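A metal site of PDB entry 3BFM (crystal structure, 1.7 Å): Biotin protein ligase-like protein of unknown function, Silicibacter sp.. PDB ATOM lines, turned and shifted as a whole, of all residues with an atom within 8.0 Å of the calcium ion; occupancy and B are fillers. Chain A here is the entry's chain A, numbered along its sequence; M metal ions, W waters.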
ATOM      1  N   ALA A  17      13.271  -4.415  27.994  1.00  0.00           N
ATOM      2  CA  ALA A  17      13.763  -3.088  27.573  1.00  0.00           C
ATOM      3  C   ALA A  17      15.095  -3.223  26.844  1.00  0.00           C
ATOM      4  O   ALA A  17      15.986  -3.984  27.262  1.00  0.00           O
ATOM      5  CB  ALA A  17      13.926  -2.173  28.801  1.00  0.00           C
ATOM      6  N   GLY A  18      15.193  -2.517  25.729  1.00  0.00           N
ATOM      7  CA  GLY A  18      16.405  -2.453  24.917  1.00  0.00           C
ATOM      8  C   GLY A  18      17.263  -1.254  25.224  1.00  0.00           C
ATOM      9  O   GLY A  18      16.993  -0.492  26.147  1.00  0.00           O
ATOM     10  N   PRO A  19      18.353  -1.110  24.460  1.00  0.00           N
ATOM     11  CA  PRO A  19      19.263   0.045  24.597  1.00  0.00           C
ATOM     12  C   PRO A  19      18.526   1.393  24.561  1.00  0.00           C
ATOM     13  O   PRO A  19      17.711   1.615  23.680  1.00  0.00           O
ATOM     14  CB  PRO A  19      20.157  -0.096  23.383  1.00  0.00           C
ATOM     15  CG  PRO A  19      20.213  -1.592  23.131  1.00  0.00           C
ATOM     16  CD  PRO A  19      18.837  -2.076  23.448  1.00  0.00           C
ATOM     17  N   GLY A  20      18.817   2.262  25.522  1.00  0.00           N
ATOM     18  CA  GLY A  20      18.215   3.558  25.563  1.00  0.00           C
ATOM     19  C   GLY A  20      16.814   3.572  26.190  1.00  0.00           C
ATOM     20  O   GLY A  20      16.242   4.634  26.359  1.00  0.00           O
ATOM     21  N   GLN A  21      16.283   2.403  26.503  1.00  0.00           N
ATOM     22  CA  GLN A  21      14.943   2.246  27.062  1.00  0.00           C
ATOM     23  C   GLN A  21      14.988   1.816  28.549  1.00  0.00           C
ATOM     24  O   GLN A  21      15.796   0.959  28.957  1.00  0.00           O
ATOM     25  CB  GLN A  21      14.169   1.188  26.276  1.00  0.00           C
ATOM     26  CG  GLN A  21      14.088   1.392  24.748  1.00  0.00           C
ATOM     27  CD  GLN A  21      13.415   0.230  23.969  1.00  0.00           C
ATOM     28  OE1 GLN A  21      13.545  -0.963  24.304  1.00  0.00           O
ATOM     29  NE2 GLN A  21      12.711   0.588  22.895  1.00  0.00           N
ATOM     30  N   ASP A  22      14.084   2.390  29.371  1.00  0.00           N
ATOM     31  CA  ASP A  22      13.828   1.865  30.714  1.00  0.00           C
ATOM     32  C   ASP A  22      12.332   1.553  30.806  1.00  0.00           C
ATOM     33  O   ASP A  22      11.526   2.174  30.108  1.00  0.00           O
ATOM     34  CB  ASP A  22      14.217   2.854  31.822  1.00  0.00           C
ATOM     35  CG  ASP A  22      15.696   3.250  31.771  1.00  0.00           C
ATOM     36  OD1 ASP A  22      16.572   2.425  31.443  1.00  0.00           O
ATOM     37  OD2 ASP A  22      15.971   4.434  32.055  1.00  0.00           O
ATOM     38  N   PRO A  23      11.963   0.546  31.608  1.00  0.00           N
ATOM     39  CA  PRO A  23      10.570   0.060  31.611  1.00  0.00           C
ATOM     40  C   PRO A  23       9.452   1.099  31.827  1.00  0.00           C
ATOM     41  O   PRO A  23       8.511   1.138  31.025  1.00  0.00           O
ATOM     42  CB  PRO A  23      10.592  -1.007  32.698  1.00  0.00           C
ATOM     43  CG  PRO A  23      11.967  -1.552  32.644  1.00  0.00           C
ATOM     44  CD  PRO A  23      12.811  -0.310  32.452  1.00  0.00           C
ATOM     45  N   TYR A  42      10.007  -4.923  31.113  1.00  0.00           N
ATOM     46  CA  TYR A  42      10.884  -5.203  32.218  1.00  0.00           C
ATOM     47  C   TYR A  42      12.348  -5.062  31.841  1.00  0.00           C
ATOM     48  O   TYR A  42      12.725  -5.039  30.654  1.00  0.00           O
ATOM     49  CB  TYR A  42      10.585  -6.594  32.796  1.00  0.00           C
ATOM     50  CG  TYR A  42      10.895  -7.729  31.819  1.00  0.00           C
ATOM     51  CD1 TYR A  42      12.143  -8.283  31.783  1.00  0.00           C
ATOM     52  CD2 TYR A  42       9.914  -8.227  30.971  1.00  0.00           C
ATOM     53  CE1 TYR A  42      12.447  -9.298  30.921  1.00  0.00           C
ATOM     54  CE2 TYR A  42      10.210  -9.272  30.081  1.00  0.00           C
ATOM     55  CZ  TYR A  42      11.454  -9.790  30.071  1.00  0.00           C
ATOM     56  OH  TYR A  42      11.780 -10.804  29.181  1.00  0.00           O
ATOM     57  N   GLU A  43      13.176  -4.914  32.860  1.00  0.00           N
ATOM     58  CA  GLU A  43      14.628  -4.800  32.676  1.00  0.00           C
ATOM     59  C   GLU A  43      15.241  -5.352  33.936  1.00  0.00           C
ATOM     60  O   GLU A  43      14.994  -4.808  35.023  1.00  0.00           O
ATOM     61  CB  GLU A  43      15.018  -3.319  32.452  1.00  0.00           C
ATOM     62  CG  GLU A  43      16.449  -3.135  32.103  1.00  0.00           C
ATOM     63  CD  GLU A  43      16.769  -1.786  31.478  1.00  0.00           C
ATOM     64  OE1 GLU A  43      16.029  -0.767  31.630  1.00  0.00           O
ATOM     65  OE2 GLU A  43      17.850  -1.692  30.878  1.00  0.00           O
ATOM     66  N   ARG A  50      13.473  -3.768  37.325  1.00  0.00           N
ATOM     67  CA  ARG A  50      12.500  -2.741  36.953  1.00  0.00           C
ATOM     68  C   ARG A  50      11.448  -3.391  36.101  1.00  0.00           C
ATOM     69  O   ARG A  50      11.774  -4.306  35.327  1.00  0.00           O
ATOM     70  CB  ARG A  50      13.126  -1.537  36.252  1.00  0.00           C
ATOM     71  CG  ARG A  50      14.025  -0.739  37.185  1.00  0.00           C
ATOM     72  CD  ARG A  50      14.795   0.320  36.413  1.00  0.00           C
ATOM     73  NE  ARG A  50      15.963  -0.274  35.807  1.00  0.00           N
ATOM     74  CZ  ARG A  50      16.742   0.319  34.920  1.00  0.00           C
ATOM     75  NH1 ARG A  50      16.484   1.546  34.470  1.00  0.00           N
ATOM     76  NH2 ARG A  50      17.796  -0.325  34.445  1.00  0.00           N
HETATM   77 CA    CA M   1      17.633   0.616  30.363  1.00  0.00          CA
HETATM   78  O   HOH W   1      18.742   2.527  29.287  1.00  0.00           O
HETATM   79  O   HOH W   2      19.379   0.881  31.959  1.00  0.00           O
HETATM   80  O   HOH W   3      18.418  -0.357  28.358  1.00  0.00           O
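The guanidinium group of Arg 50 lies within salt-bridge range of the side-chain carboxylate of Asp 22. O of Arg 50 is in hydrogen-bond range of N of Glu 43. The side-chain amide oxygen of Gln 21 is in hydrogen-bond range of the backbone NH of Gly 18 (2.7 Å).
Of the 10 residues printed, 3 come within 4 Å of the calcium ion.
The calcium ion is bound by O of Gln 21, OD1 of Asp 22, water W3, OE2 of Glu 43, water W2, water W1 and OE1 of Glu 43.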
